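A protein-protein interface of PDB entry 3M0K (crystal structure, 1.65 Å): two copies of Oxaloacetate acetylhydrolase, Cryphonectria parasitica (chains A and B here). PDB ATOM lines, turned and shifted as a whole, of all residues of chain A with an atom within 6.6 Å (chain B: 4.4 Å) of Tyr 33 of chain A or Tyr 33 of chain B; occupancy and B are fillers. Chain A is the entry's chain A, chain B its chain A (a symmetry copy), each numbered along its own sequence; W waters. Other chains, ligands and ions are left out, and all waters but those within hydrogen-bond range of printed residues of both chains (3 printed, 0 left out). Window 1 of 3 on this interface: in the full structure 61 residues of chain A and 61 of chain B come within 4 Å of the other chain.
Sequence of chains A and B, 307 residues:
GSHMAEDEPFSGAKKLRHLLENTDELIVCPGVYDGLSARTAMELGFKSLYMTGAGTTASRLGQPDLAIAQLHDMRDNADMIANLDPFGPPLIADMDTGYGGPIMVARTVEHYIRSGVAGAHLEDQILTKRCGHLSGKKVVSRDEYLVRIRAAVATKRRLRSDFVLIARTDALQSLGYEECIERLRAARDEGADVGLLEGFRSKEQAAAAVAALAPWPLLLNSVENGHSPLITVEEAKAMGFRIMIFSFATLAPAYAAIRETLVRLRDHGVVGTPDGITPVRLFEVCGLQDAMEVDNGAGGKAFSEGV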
ATOM      1  N   GLY A  31      -5.088 -32.324 -20.130  1.00  0.00           N
ATOM      2  CA  GLY A  31      -3.827 -32.739 -20.698  1.00  0.00           C
ATOM      3  C   GLY A  31      -2.877 -31.561 -20.775  1.00  0.00           C
ATOM      4  O   GLY A  31      -3.150 -30.569 -21.464  1.00  0.00           O
ATOM      5  N   VAL A  32      -1.762 -31.686 -20.065  1.00  0.00           N
ATOM      6  CA  VAL A  32      -0.731 -30.652 -20.017  1.00  0.00           C
ATOM      7  C   VAL A  32       0.570 -31.189 -20.599  1.00  0.00           C
ATOM      8  O   VAL A  32       0.765 -32.404 -20.687  1.00  0.00           O
ATOM      9  CB  VAL A  32      -0.516 -30.156 -18.581  1.00  0.00           C
ATOM     10  CG1 VAL A  32      -1.832 -29.625 -18.032  1.00  0.00           C
ATOM     11  CG2 VAL A  32       0.035 -31.286 -17.676  1.00  0.00           C
ATOM     12  N   TYR A  33       1.477 -30.296 -20.986  1.00  0.00           N
ATOM     13  CA  TYR A  33       2.616 -30.741 -21.773  1.00  0.00           C
ATOM     14  C   TYR A  33       3.909 -30.007 -21.456  1.00  0.00           C
ATOM     15  O   TYR A  33       4.970 -30.334 -21.988  1.00  0.00           O
ATOM     16  CB  TYR A  33       2.297 -30.585 -23.254  1.00  0.00           C
ATOM     17  CG  TYR A  33       2.125 -29.145 -23.691  1.00  0.00           C
ATOM     18  CD1 TYR A  33       3.208 -28.407 -24.136  1.00  0.00           C
ATOM     19  CD2 TYR A  33       0.878 -28.531 -23.663  1.00  0.00           C
ATOM     20  CE1 TYR A  33       3.052 -27.084 -24.555  1.00  0.00           C
ATOM     21  CE2 TYR A  33       0.707 -27.223 -24.069  1.00  0.00           C
ATOM     22  CZ  TYR A  33       1.801 -26.506 -24.524  1.00  0.00           C
ATOM     23  OH  TYR A  33       1.634 -25.204 -24.937  1.00  0.00           O
ATOM     24  N   ASP A  34       3.813 -28.986 -20.621  1.00  0.00           N
ATOM     25  CA  ASP A  34       4.995 -28.231 -20.230  1.00  0.00           C
ATOM     26  C   ASP A  34       4.703 -27.539 -18.909  1.00  0.00           C
ATOM     27  O   ASP A  34       3.669 -27.783 -18.289  1.00  0.00           O
ATOM     28  CB  ASP A  34       5.410 -27.228 -21.310  1.00  0.00           C
ATOM     29  CG  ASP A  34       4.497 -26.025 -21.383  1.00  0.00           C
ATOM     30  OD1 ASP A  34       3.336 -26.120 -20.934  1.00  0.00           O
ATOM     31  OD2 ASP A  34       4.937 -24.980 -21.911  1.00  0.00           O
ATOM     32  N   GLY A  35       5.619 -26.686 -18.474  1.00  0.00           N
ATOM     33  CA  GLY A  35       5.484 -26.031 -17.189  1.00  0.00           C
ATOM     34  C   GLY A  35       4.359 -25.022 -17.185  1.00  0.00           C
ATOM     35  O   GLY A  35       3.659 -24.878 -16.190  1.00  0.00           O
ATOM     36  N   LEU A  36       4.187 -24.328 -18.302  1.00  0.00           N
ATOM     37  CA  LEU A  36       3.174 -23.285 -18.378  1.00  0.00           C
ATOM     38  C   LEU A  36       1.779 -23.892 -18.381  1.00  0.00           C
ATOM     39  O   LEU A  36       0.906 -23.441 -17.652  1.00  0.00           O
ATOM     40  CB  LEU A  36       3.377 -22.410 -19.611  1.00  0.00           C
ATOM     41  CG  LEU A  36       2.326 -21.308 -19.753  1.00  0.00           C
ATOM     42  CD1 LEU A  36       2.430 -20.321 -18.572  1.00  0.00           C
ATOM     43  CD2 LEU A  36       2.465 -20.616 -21.090  1.00  0.00           C
ATOM     44  N   SER A  37       1.559 -24.901 -19.214  1.00  0.00           N
ATOM     45  CA  SER A  37       0.259 -25.549 -19.234  1.00  0.00           C
ATOM     46  C   SER A  37      -0.041 -26.204 -17.878  1.00  0.00           C
ATOM     47  O   SER A  37      -1.152 -26.078 -17.356  1.00  0.00           O
ATOM     48  CB  SER A  37       0.146 -26.540 -20.390  1.00  0.00           C
ATOM     49  OG  SER A  37       1.185 -27.503 -20.333  1.00  0.00           O
ATOM     50  N   ALA A  38       0.952 -26.869 -17.288  1.00  0.00           N
ATOM     51  CA  ALA A  38       0.720 -27.497 -15.994  1.00  0.00           C
ATOM     52  C   ALA A  38       0.417 -26.454 -14.912  1.00  0.00           C
ATOM     53  O   ALA A  38      -0.485 -26.642 -14.099  1.00  0.00           O
ATOM     54  CB  ALA A  38       1.916 -28.379 -15.592  1.00  0.00           C
ATOM     55  N   TYR A  50      -2.961 -34.577 -16.460  1.00  0.00           N
ATOM     56  CA  TYR A  50      -2.511 -35.613 -17.358  1.00  0.00           C
ATOM     57  C   TYR A  50      -1.379 -35.089 -18.230  1.00  0.00           C
ATOM     58  O   TYR A  50      -1.497 -34.030 -18.835  1.00  0.00           O
ATOM     59  CB  TYR A  50      -3.669 -36.087 -18.234  1.00  0.00           C
ATOM     60  CG  TYR A  50      -3.195 -36.959 -19.372  1.00  0.00           C
ATOM     61  CD1 TYR A  50      -2.580 -38.179 -19.126  1.00  0.00           C
ATOM     62  CD2 TYR A  50      -3.344 -36.559 -20.692  1.00  0.00           C
ATOM     63  CE1 TYR A  50      -2.131 -38.978 -20.157  1.00  0.00           C
ATOM     64  CE2 TYR A  50      -2.895 -37.359 -21.728  1.00  0.00           C
ATOM     65  CZ  TYR A  50      -2.290 -38.564 -21.454  1.00  0.00           C
ATOM     66  OH  TYR A  50      -1.863 -39.345 -22.488  1.00  0.00           O
ATOM     67  N   MET A  51      -0.270 -35.818 -18.290  1.00  0.00           N
ATOM     68  CA  MET A  51       0.803 -35.401 -19.185  1.00  0.00           C
ATOM     69  C   MET A  51       0.711 -36.170 -20.481  1.00  0.00           C
ATOM     70  O   MET A  51       0.938 -37.375 -20.502  1.00  0.00           O
ATOM     71  CB  MET A  51       2.188 -35.620 -18.570  1.00  0.00           C
ATOM     72  CG  MET A  51       3.307 -35.036 -19.440  1.00  0.00           C
ATOM     73  SD  MET A  51       4.959 -35.496 -18.884  1.00  0.00           S
ATOM     74  CE  MET A  51       5.159 -37.021 -19.816  1.00  0.00           C
ATOM     75  N   THR A  52       0.372 -35.463 -21.557  1.00  0.00           N
ATOM     76  CA  THR A  52       0.288 -36.047 -22.881  1.00  0.00           C
ATOM     77  C   THR A  52       1.663 -36.342 -23.474  1.00  0.00           C
ATOM     78  O   THR A  52       2.590 -35.522 -23.381  1.00  0.00           O
ATOM     79  CB  THR A  52      -0.477 -35.096 -23.839  1.00  0.00           C
ATOM     80  OG1 THR A  52      -0.224 -35.465 -25.195  1.00  0.00           O
ATOM     81  CG2 THR A  52      -0.025 -33.666 -23.661  1.00  0.00           C
ATOM     82  N   ALA A  54       1.998 -36.937 -26.835  1.00  0.00           N
ATOM     83  CA  ALA A  54       1.995 -36.131 -28.049  1.00  0.00           C
ATOM     84  C   ALA A  54       2.417 -34.703 -27.734  1.00  0.00           C
ATOM     85  O   ALA A  54       3.228 -34.117 -28.460  1.00  0.00           O
ATOM     86  CB  ALA A  54       0.626 -36.149 -28.708  1.00  0.00           C
ATOM     87  N   GLY A  55       1.863 -34.140 -26.662  1.00  0.00           N
ATOM     88  CA  GLY A  55       2.202 -32.773 -26.276  1.00  0.00           C
ATOM     89  C   GLY A  55       3.651 -32.644 -25.837  1.00  0.00           C
ATOM     90  O   GLY A  55       4.344 -31.692 -26.187  1.00  0.00           O
ATOM     91  N   THR A  56       4.119 -33.615 -25.063  1.00  0.00           N
ATOM     92  CA  THR A  56       5.495 -33.610 -24.613  1.00  0.00           C
ATOM     93  C   THR A  56       6.435 -33.630 -25.819  1.00  0.00           C
ATOM     94  O   THR A  56       7.414 -32.888 -25.866  1.00  0.00           O
ATOM     95  CB  THR A  56       5.787 -34.806 -23.669  1.00  0.00           C
ATOM     96  OG1 THR A  56       4.979 -34.693 -22.486  1.00  0.00           O
ATOM     97  CG2 THR A  56       7.268 -34.828 -23.277  1.00  0.00           C
ATOM     98  N   THR A  57       6.120 -34.461 -26.807  1.00  0.00           N
ATOM     99  CA  THR A  57       6.950 -34.564 -28.002  1.00  0.00           C
ATOM    100  C   THR A  57       6.938 -33.262 -28.816  1.00  0.00           C
ATOM    101  O   THR A  57       7.984 -32.785 -29.269  1.00  0.00           O
ATOM    102  CB  THR A  57       6.499 -35.735 -28.876  1.00  0.00           C
ATOM    103  OG1 THR A  57       6.430 -36.927 -28.077  1.00  0.00           O
ATOM    104  CG2 THR A  57       7.486 -35.948 -30.004  1.00  0.00           C
ATOM    105  N   ALA A  58       5.757 -32.682 -28.990  1.00  0.00           N
ATOM    106  CA  ALA A  58       5.644 -31.425 -29.732  1.00  0.00           C
ATOM    107  C   ALA A  58       6.415 -30.299 -29.056  1.00  0.00           C
ATOM    108  O   ALA A  58       7.149 -29.558 -29.715  1.00  0.00           O
ATOM    109  CB  ALA A  58       4.173 -31.038 -29.904  1.00  0.00           C
ATOM    110  N   SER A  59       6.271 -30.182 -27.738  1.00  0.00           N
ATOM    111  CA  SER A  59       6.846 -29.065 -26.993  1.00  0.00           C
ATOM    112  C   SER A  59       8.330 -29.258 -26.660  1.00  0.00           C
ATOM    113  O   SER A  59       9.145 -28.374 -26.899  1.00  0.00           O
ATOM    114  CB  SER A  59       6.054 -28.833 -25.706  1.00  0.00           C
ATOM    115  OG  SER A  59       6.630 -27.795 -24.927  1.00  0.00           O
ATOM    116  N   ARG A  60       8.683 -30.405 -26.089  1.00  0.00           N
ATOM    117  CA  ARG A  60      10.073 -30.631 -25.721  1.00  0.00           C
ATOM    118  C   ARG A  60      10.974 -30.938 -26.915  1.00  0.00           C
ATOM    119  O   ARG A  60      12.189 -30.683 -26.867  1.00  0.00           O
ATOM    120  CB  ARG A  60      10.172 -31.761 -24.703  1.00  0.00           C
ATOM    121  CG  ARG A  60       9.726 -31.355 -23.317  1.00  0.00           C
ATOM    122  CD  ARG A  60       9.969 -32.471 -22.319  1.00  0.00           C
ATOM    123  NE  ARG A  60      11.391 -32.712 -22.091  1.00  0.00           N
ATOM    124  CZ  ARG A  60      12.115 -32.081 -21.170  1.00  0.00           C
ATOM    125  NH1 ARG A  60      11.553 -31.161 -20.395  1.00  0.00           N
ATOM    126  NH2 ARG A  60      13.402 -32.369 -21.026  1.00  0.00           N
ATOM    127  N   ASN A  77      10.020 -34.660 -18.357  1.00  0.00           N
ATOM    128  CA  ASN A  77       8.847 -33.797 -18.378  1.00  0.00           C
ATOM    129  C   ASN A  77       7.915 -34.120 -17.214  1.00  0.00           C
ATOM    130  O   ASN A  77       7.376 -33.227 -16.566  1.00  0.00           O
ATOM    131  CB  ASN A  77       8.091 -33.916 -19.696  1.00  0.00           C
ATOM    132  CG  ASN A  77       7.440 -32.607 -20.103  1.00  0.00           C
ATOM    133  OD1 ASN A  77       7.959 -31.535 -19.807  1.00  0.00           O
ATOM    134  ND2 ASN A  77       6.314 -32.687 -20.797  1.00  0.00           N
ATOM    135  N   MET A  80       9.357 -32.984 -13.880  1.00  0.00           N
ATOM    136  CA  MET A  80       9.141 -31.546 -13.764  1.00  0.00           C
ATOM    137  C   MET A  80       7.696 -31.215 -13.377  1.00  0.00           C
ATOM    138  O   MET A  80       7.446 -30.496 -12.409  1.00  0.00           O
ATOM    139  CB  MET A  80       9.523 -30.842 -15.064  1.00  0.00           C
ATOM    140  CG  MET A  80       9.410 -29.311 -14.970  1.00  0.00           C
ATOM    141  SD  MET A  80       7.787 -28.733 -15.455  1.00  0.00           S
ATOM    142  CE  MET A  80       7.766 -29.154 -17.200  1.00  0.00           C
ATOM    143  N   ILE A  81       6.741 -31.746 -14.122  1.00  0.00           N
ATOM    144  CA  ILE A  81       5.354 -31.360 -13.897  1.00  0.00           C
ATOM    145  C   ILE A  81       4.813 -31.861 -12.555  1.00  0.00           C
ATOM    146  O   ILE A  81       4.179 -31.109 -11.811  1.00  0.00           O
ATOM    147  CB  ILE A  81       4.458 -31.819 -15.061  1.00  0.00           C
ATOM    148  CG1 ILE A  81       4.837 -31.068 -16.348  1.00  0.00           C
ATOM    149  CG2 ILE A  81       2.990 -31.610 -14.698  1.00  0.00           C
ATOM    150  CD1 ILE A  81       4.332 -31.752 -17.657  1.00  0.00           C
ATOM    151  N   THR A 250      -4.652 -28.396 -23.877  1.00  0.00           N
ATOM    152  CA  THR A 250      -3.832 -27.193 -23.792  1.00  0.00           C
ATOM    153  C   THR A 250      -2.951 -26.997 -25.029  1.00  0.00           C
ATOM    154  O   THR A 250      -2.718 -25.869 -25.455  1.00  0.00           O
ATOM    155  CB  THR A 250      -2.997 -27.157 -22.502  1.00  0.00           C
ATOM    156  OG1 THR A 250      -2.124 -28.283 -22.461  1.00  0.00           O
ATOM    157  CG2 THR A 250      -3.903 -27.197 -21.276  1.00  0.00           C
ATOM    158  N   LEU A 251      -2.489 -28.088 -25.630  1.00  0.00           N
ATOM    159  CA  LEU A 251      -1.612 -27.968 -26.792  1.00  0.00           C
ATOM    160  C   LEU A 251      -2.348 -27.293 -27.952  1.00  0.00           C
ATOM    161  O   LEU A 251      -1.814 -26.399 -28.618  1.00  0.00           O
ATOM    162  CB  LEU A 251      -1.085 -29.339 -27.213  1.00  0.00           C
ATOM    163  CG  LEU A 251       0.054 -29.294 -28.229  1.00  0.00           C
ATOM    164  CD1 LEU A 251       1.358 -28.873 -27.537  1.00  0.00           C
ATOM    165  CD2 LEU A 251       0.214 -30.658 -28.887  1.00  0.00           C
ATOM    166  N   ALA A 252      -3.582 -27.718 -28.187  1.00  0.00           N
ATOM    167  CA  ALA A 252      -4.353 -27.179 -29.297  1.00  0.00           C
ATOM    168  C   ALA A 252      -4.667 -25.673 -29.177  1.00  0.00           C
ATOM    169  O   ALA A 252      -4.376 -24.922 -30.100  1.00  0.00           O
ATOM    170  CB  ALA A 252      -5.623 -27.996 -29.527  1.00  0.00           C
ATOM    171  N   ALA A 254      -3.131 -23.568 -27.385  1.00  0.00           N
ATOM    172  CA  ALA A 254      -1.851 -22.876 -27.384  1.00  0.00           C
ATOM    173  C   ALA A 254      -1.422 -22.612 -28.818  1.00  0.00           C
ATOM    174  O   ALA A 254      -1.013 -21.505 -29.142  1.00  0.00           O
ATOM    175  CB  ALA A 254      -0.768 -23.672 -26.639  1.00  0.00           C
ATOM    176  N   TYR A 255      -1.521 -23.634 -29.669  1.00  0.00           N
ATOM    177  CA  TYR A 255      -1.142 -23.478 -31.062  1.00  0.00           C
ATOM    178  C   TYR A 255      -1.977 -22.418 -31.770  1.00  0.00           C
ATOM    179  O   TYR A 255      -1.429 -21.543 -32.439  1.00  0.00           O
ATOM    180  CB  TYR A 255      -1.239 -24.792 -31.832  1.00  0.00           C
ATOM    181  CG  TYR A 255      -1.080 -24.576 -33.327  1.00  0.00           C
ATOM    182  CD1 TYR A 255       0.169 -24.332 -33.882  1.00  0.00           C
ATOM    183  CD2 TYR A 255      -2.178 -24.595 -34.175  1.00  0.00           C
ATOM    184  CE1 TYR A 255       0.319 -24.121 -35.245  1.00  0.00           C
ATOM    185  CE2 TYR A 255      -2.040 -24.384 -35.533  1.00  0.00           C
ATOM    186  CZ  TYR A 255      -0.790 -24.150 -36.066  1.00  0.00           C
ATOM    187  OH  TYR A 255      -0.648 -23.944 -37.424  1.00  0.00           O
ATOM    188  N   ILE A 258      -0.918 -18.941 -30.478  1.00  0.00           N
ATOM    189  CA  ILE A 258       0.423 -18.591 -30.926  1.00  0.00           C
ATOM    190  C   ILE A 258       0.375 -18.237 -32.403  1.00  0.00           C
ATOM    191  O   ILE A 258       0.960 -17.249 -32.840  1.00  0.00           O
ATOM    192  CB  ILE A 258       1.418 -19.763 -30.708  1.00  0.00           C
ATOM    193  CG1 ILE A 258       1.647 -19.991 -29.208  1.00  0.00           C
ATOM    194  CG2 ILE A 258       2.732 -19.484 -31.433  1.00  0.00           C
ATOM    195  CD1 ILE A 258       2.269 -21.355 -28.863  1.00  0.00           C
ATOM    196  N   VAL B  32      10.241 -17.391 -29.102  1.00  0.00           N
ATOM    197  CA  VAL B  32       9.716 -18.750 -28.993  1.00  0.00           C
ATOM    198  C   VAL B  32      10.354 -19.460 -27.806  1.00  0.00           C
ATOM    199  O   VAL B  32      11.416 -19.052 -27.327  1.00  0.00           O
ATOM    200  CB  VAL B  32       9.956 -19.539 -30.287  1.00  0.00           C
ATOM    201  CG1 VAL B  32       9.303 -18.804 -31.449  1.00  0.00           C
ATOM    202  CG2 VAL B  32      11.469 -19.736 -30.548  1.00  0.00           C
ATOM    203  N   TYR B  33       9.728 -20.534 -27.332  1.00  0.00           N
ATOM    204  CA  TYR B  33      10.152 -21.093 -26.058  1.00  0.00           C
ATOM    205  C   TYR B  33      10.077 -22.610 -25.995  1.00  0.00           C
ATOM    206  O   TYR B  33      10.480 -23.224 -25.006  1.00  0.00           O
ATOM    207  CB  TYR B  33       9.305 -20.499 -24.940  1.00  0.00           C
ATOM    208  CG  TYR B  33       7.843 -20.889 -25.012  1.00  0.00           C
ATOM    209  CD1 TYR B  33       7.382 -22.027 -24.373  1.00  0.00           C
ATOM    210  CD2 TYR B  33       6.927 -20.113 -25.714  1.00  0.00           C
ATOM    211  CE1 TYR B  33       6.033 -22.382 -24.423  1.00  0.00           C
ATOM    212  CE2 TYR B  33       5.591 -20.453 -25.778  1.00  0.00           C
ATOM    213  CZ  TYR B  33       5.148 -21.588 -25.120  1.00  0.00           C
ATOM    214  OH  TYR B  33       3.815 -21.925 -25.174  1.00  0.00           O
ATOM    215  N   ASP B  34       9.522 -23.212 -27.032  1.00  0.00           N
ATOM    216  CA  ASP B  34       9.424 -24.664 -27.086  1.00  0.00           C
ATOM    217  C   ASP B  34       9.285 -25.079 -28.541  1.00  0.00           C
ATOM    218  O   ASP B  34       9.413 -24.253 -29.443  1.00  0.00           O
ATOM    219  CB  ASP B  34       8.259 -25.185 -26.240  1.00  0.00           C
ATOM    220  CG  ASP B  34       6.909 -24.934 -26.871  1.00  0.00           C
ATOM    221  OD1 ASP B  34       6.798 -24.021 -27.718  1.00  0.00           O
ATOM    222  OD2 ASP B  34       5.944 -25.641 -26.508  1.00  0.00           O
ATOM    223  N   SER B  37       5.894 -23.517 -30.273  1.00  0.00           N
ATOM    224  CA  SER B  37       6.016 -22.112 -30.620  1.00  0.00           C
ATOM    225  C   SER B  37       7.036 -21.919 -31.751  1.00  0.00           C
ATOM    226  O   SER B  37       6.784 -21.169 -32.698  1.00  0.00           O
ATOM    227  CB  SER B  37       6.346 -21.260 -29.396  1.00  0.00           C
ATOM    228  OG  SER B  37       7.526 -21.723 -28.761  1.00  0.00           O
ATOM    229  N   THR B  52      13.533 -17.101 -25.919  1.00  0.00           N
ATOM    230  CA  THR B  52      13.456 -16.414 -24.645  1.00  0.00           C
ATOM    231  C   THR B  52      13.908 -17.294 -23.482  1.00  0.00           C
ATOM    232  O   THR B  52      13.549 -18.479 -23.399  1.00  0.00           O
ATOM    233  CB  THR B  52      12.003 -15.940 -24.378  1.00  0.00           C
ATOM    234  OG1 THR B  52      11.840 -15.629 -22.994  1.00  0.00           O
ATOM    235  CG2 THR B  52      11.006 -17.019 -24.727  1.00  0.00           C
ATOM    236  N   GLY B  55      10.783 -17.616 -21.207  1.00  0.00           N
ATOM    237  CA  GLY B  55       9.889 -18.626 -21.765  1.00  0.00           C
ATOM    238  C   GLY B  55      10.430 -20.034 -21.584  1.00  0.00           C
ATOM    239  O   GLY B  55       9.700 -20.963 -21.246  1.00  0.00           O
ATOM    240  N   THR B  56      11.728 -20.198 -21.808  1.00  0.00           N
ATOM    241  CA  THR B  56      12.356 -21.491 -21.633  1.00  0.00           C
ATOM    242  C   THR B  56      12.180 -21.962 -20.189  1.00  0.00           C
ATOM    243  O   THR B  56      11.847 -23.119 -19.941  1.00  0.00           O
ATOM    244  CB  THR B  56      13.858 -21.448 -22.018  1.00  0.00           C
ATOM    245  OG1 THR B  56      13.988 -21.125 -23.413  1.00  0.00           O
ATOM    246  CG2 THR B  56      14.520 -22.803 -21.743  1.00  0.00           C
ATOM    247  N   SER B  59       8.400 -22.875 -19.499  1.00  0.00           N
ATOM    248  CA  SER B  59       7.943 -24.068 -20.207  1.00  0.00           C
ATOM    249  C   SER B  59       8.726 -25.331 -19.834  1.00  0.00           C
ATOM    250  O   SER B  59       8.140 -26.363 -19.524  1.00  0.00           O
ATOM    251  CB  SER B  59       8.020 -23.840 -21.717  1.00  0.00           C
ATOM    252  OG  SER B  59       7.645 -25.007 -22.434  1.00  0.00           O
ATOM    253  N   ASN B  77      17.299 -26.526 -24.940  1.00  0.00           N
ATOM    254  CA  ASN B  77      16.175 -25.913 -25.634  1.00  0.00           C
ATOM    255  C   ASN B  77      16.629 -25.282 -26.948  1.00  0.00           C
ATOM    256  O   ASN B  77      15.961 -25.400 -27.971  1.00  0.00           O
ATOM    257  CB  ASN B  77      15.487 -24.866 -24.765  1.00  0.00           C
ATOM    258  CG  ASN B  77      13.994 -24.797 -25.027  1.00  0.00           C
ATOM    259  OD1 ASN B  77      13.372 -25.803 -25.355  1.00  0.00           O
ATOM    260  ND2 ASN B  77      13.410 -23.618 -24.866  1.00  0.00           N
ATOM    261  N   ILE B  81      15.502 -26.178 -30.756  1.00  0.00           N
ATOM    262  CA  ILE B  81      14.817 -25.232 -31.626  1.00  0.00           C
ATOM    263  C   ILE B  81      15.622 -24.900 -32.887  1.00  0.00           C
ATOM    264  O   ILE B  81      15.083 -24.899 -33.996  1.00  0.00           O
ATOM    265  CB  ILE B  81      14.436 -23.952 -30.860  1.00  0.00           C
ATOM    266  CG1 ILE B  81      13.390 -24.274 -29.781  1.00  0.00           C
ATOM    267  CG2 ILE B  81      13.933 -22.894 -31.838  1.00  0.00           C
ATOM    268  CD1 ILE B  81      13.267 -23.187 -28.668  1.00  0.00           C
ATOM    269  N   THR B 250       4.930 -15.411 -27.845  1.00  0.00           N
ATOM    270  CA  THR B 250       4.207 -16.676 -27.900  1.00  0.00           C
ATOM    271  C   THR B 250       3.816 -17.187 -26.510  1.00  0.00           C
ATOM    272  O   THR B 250       2.756 -17.783 -26.342  1.00  0.00           O
ATOM    273  CB  THR B 250       4.980 -17.745 -28.689  1.00  0.00           C
ATOM    274  OG1 THR B 250       6.238 -17.989 -28.066  1.00  0.00           O
ATOM    275  CG2 THR B 250       5.226 -17.281 -30.121  1.00  0.00           C
ATOM    276  N   LEU B 251       4.646 -16.926 -25.507  1.00  0.00           N
ATOM    277  CA  LEU B 251       4.349 -17.419 -24.164  1.00  0.00           C
ATOM    278  C   LEU B 251       3.057 -16.790 -23.636  1.00  0.00           C
ATOM    279  O   LEU B 251       2.195 -17.473 -23.072  1.00  0.00           O
ATOM    280  CB  LEU B 251       5.513 -17.135 -23.216  1.00  0.00           C
ATOM    281  CG  LEU B 251       5.425 -17.855 -21.873  1.00  0.00           C
ATOM    282  CD1 LEU B 251       5.775 -19.339 -22.049  1.00  0.00           C
ATOM    283  CD2 LEU B 251       6.366 -17.199 -20.871  1.00  0.00           C
ATOM    284  N   ALA B 254      -0.133 -17.962 -25.441  1.00  0.00           N
ATOM    285  CA  ALA B 254      -0.307 -19.365 -25.097  1.00  0.00           C
ATOM    286  C   ALA B 254      -0.984 -19.469 -23.741  1.00  0.00           C
ATOM    287  O   ALA B 254      -1.928 -20.232 -23.583  1.00  0.00           O
ATOM    288  CB  ALA B 254       1.030 -20.123 -25.088  1.00  0.00           C
ATOM    289  N   ILE B 258      -4.630 -21.121 -23.060  1.00  0.00           N
ATOM    290  CA  ILE B 258      -4.678 -22.302 -22.210  1.00  0.00           C
ATOM    291  C   ILE B 258      -5.604 -22.030 -21.036  1.00  0.00           C
ATOM    292  O   ILE B 258      -6.436 -22.860 -20.676  1.00  0.00           O
ATOM    293  CB  ILE B 258      -3.268 -22.676 -21.678  1.00  0.00           C
ATOM    294  CG1 ILE B 258      -2.381 -23.165 -22.829  1.00  0.00           C
ATOM    295  CG2 ILE B 258      -3.378 -23.729 -20.578  1.00  0.00           C
ATOM    296  CD1 ILE B 258      -0.875 -23.168 -22.512  1.00  0.00           C
HETATM  297  O   HOH W   1       2.983 -23.475 -23.180  1.00  0.00           O
HETATM  298  O   HOH W   2       8.733 -27.427 -23.183  1.00  0.00           O
HETATM  299  O   HOH W   3       3.505 -24.323 -26.607  1.00  0.00           O
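Tyr 33 of chain A touches just these residues of chain B: Tyr 33 and Asp 34.
Of chain A, only Tyr 33 and Asp 34 come within 4 Å of Tyr 33 of chain B.
Printed residues of chain A within 4 Å of Asp 34 of chain B: Tyr 33 and Ser 59.
Of the printed residues of chain A, Thr 250 of chain B touches Ile 258 (3.6 Å).
Printed residues of chain B within 4 Å of Leu 36 of chain A: Leu 251 (3.7 Å).
Ala 54 of chain A touches none of the printed residues of chain B.
The nearest printed residue of chain B that does not touch Met 80 of chain A is Thr 56 of chain B (7.8 Å).
OG1 of Thr 250 of chain A is in hydrogen-bond range of O of Gly 31 of chain A, at 2.7 Å.
The backbone NH of Tyr 33 of chain A is in hydrogen-bond range of the side-chain hydroxyl of Ser 37 of chain A (2.9 Å).
The backbone NH (N) of Leu 36 of chain A sits at hydrogen-bond distance from the side-chain carboxylate (OD1) of Asp 34 of chain A, 3.3 Å away.
Tyr 33 of chain A touches its own counterpart, Tyr 33 of chain B.
Asp 34 of chain A touches Ser 59 of chain B, and with the chains exchanged Ser 59 of chain A touches Asp 34 of chain B.
Thr 250 of chain A touches Ile 258 of chain B, and with the chains exchanged Ile 258 of chain A touches Thr 250 of chain B.
Of the 11 pairs that touch across the chains among the printed residues, 8 have their exchanged pair printed and touching as well.
Water W3 lies within hydrogen-bond range of the side-chain hydroxyl (OH) of Tyr 33 of chain A, the side-chain carboxylate (OD2) of Asp 34 of chain B and the side-chain hydroxyl (OH) of Tyr 33 of chain B.
Water W1 lies within hydrogen-bond range of OH of Tyr 33 of chain B (2.7 Å), OD2 of Asp 34 of chain A (2.8 Å) and OH of Tyr 33 of chain A (2.8 Å).
Water W2 lies within hydrogen-bond range of the side-chain hydroxyl of Ser 59 of chain A (2.8 Å) and the side-chain hydroxyl of Ser 59 of chain B (2.8 Å).
The side-chain hydroxyl of Ser 59 of chain B is in hydrogen-bond range of the side-chain carboxylate of Asp 34 of chain A.
The backbone carbonyl oxygen (O) of Ser 59 of chain B lies within hydrogen-bond range of the backbone NH (N) of Gly 35 of chain A (2.7 Å).
The side-chain carboxylate (OD2) of Asp 34 of chain B lies within hydrogen-bond range of the side-chain hydroxyl (OG) of Ser 59 of chain A.
Of the 14 printed residues of chain B, 6 touch a printed residue of chain A.
Hydrophobic or aromatic side chains of chain B that line the printed part of chain A: Tyr 33, Leu 251 and Ile 258.
Of the 27 printed residues of chain A, 8 touch a printed residue of chain B.
Hydrophobic or aromatic side chains of chain A that line the printed part of chain B: Tyr 33, Leu 36, Met 80 and Ile 258.
Among the printed residues, 11 pairs touch across the chains.
Among the printed residues, pairs that only touch across the chains: Tyr 33 of chain A with Tyr 33 of chain B, Tyr 33 of chain A with Asp 34 of chain B, Asp 34 of chain A with Tyr 33 of chain B, Leu 36 of chain A with Leu 251 of chain B, Ser 59 of chain A with Ser 59 of chain B, Met 80 of chain A with Ser 59 of chain B, Thr 250 of chain A with Ile 258 of chain B and Ile 258 of chain A with Thr 250 of chain B.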
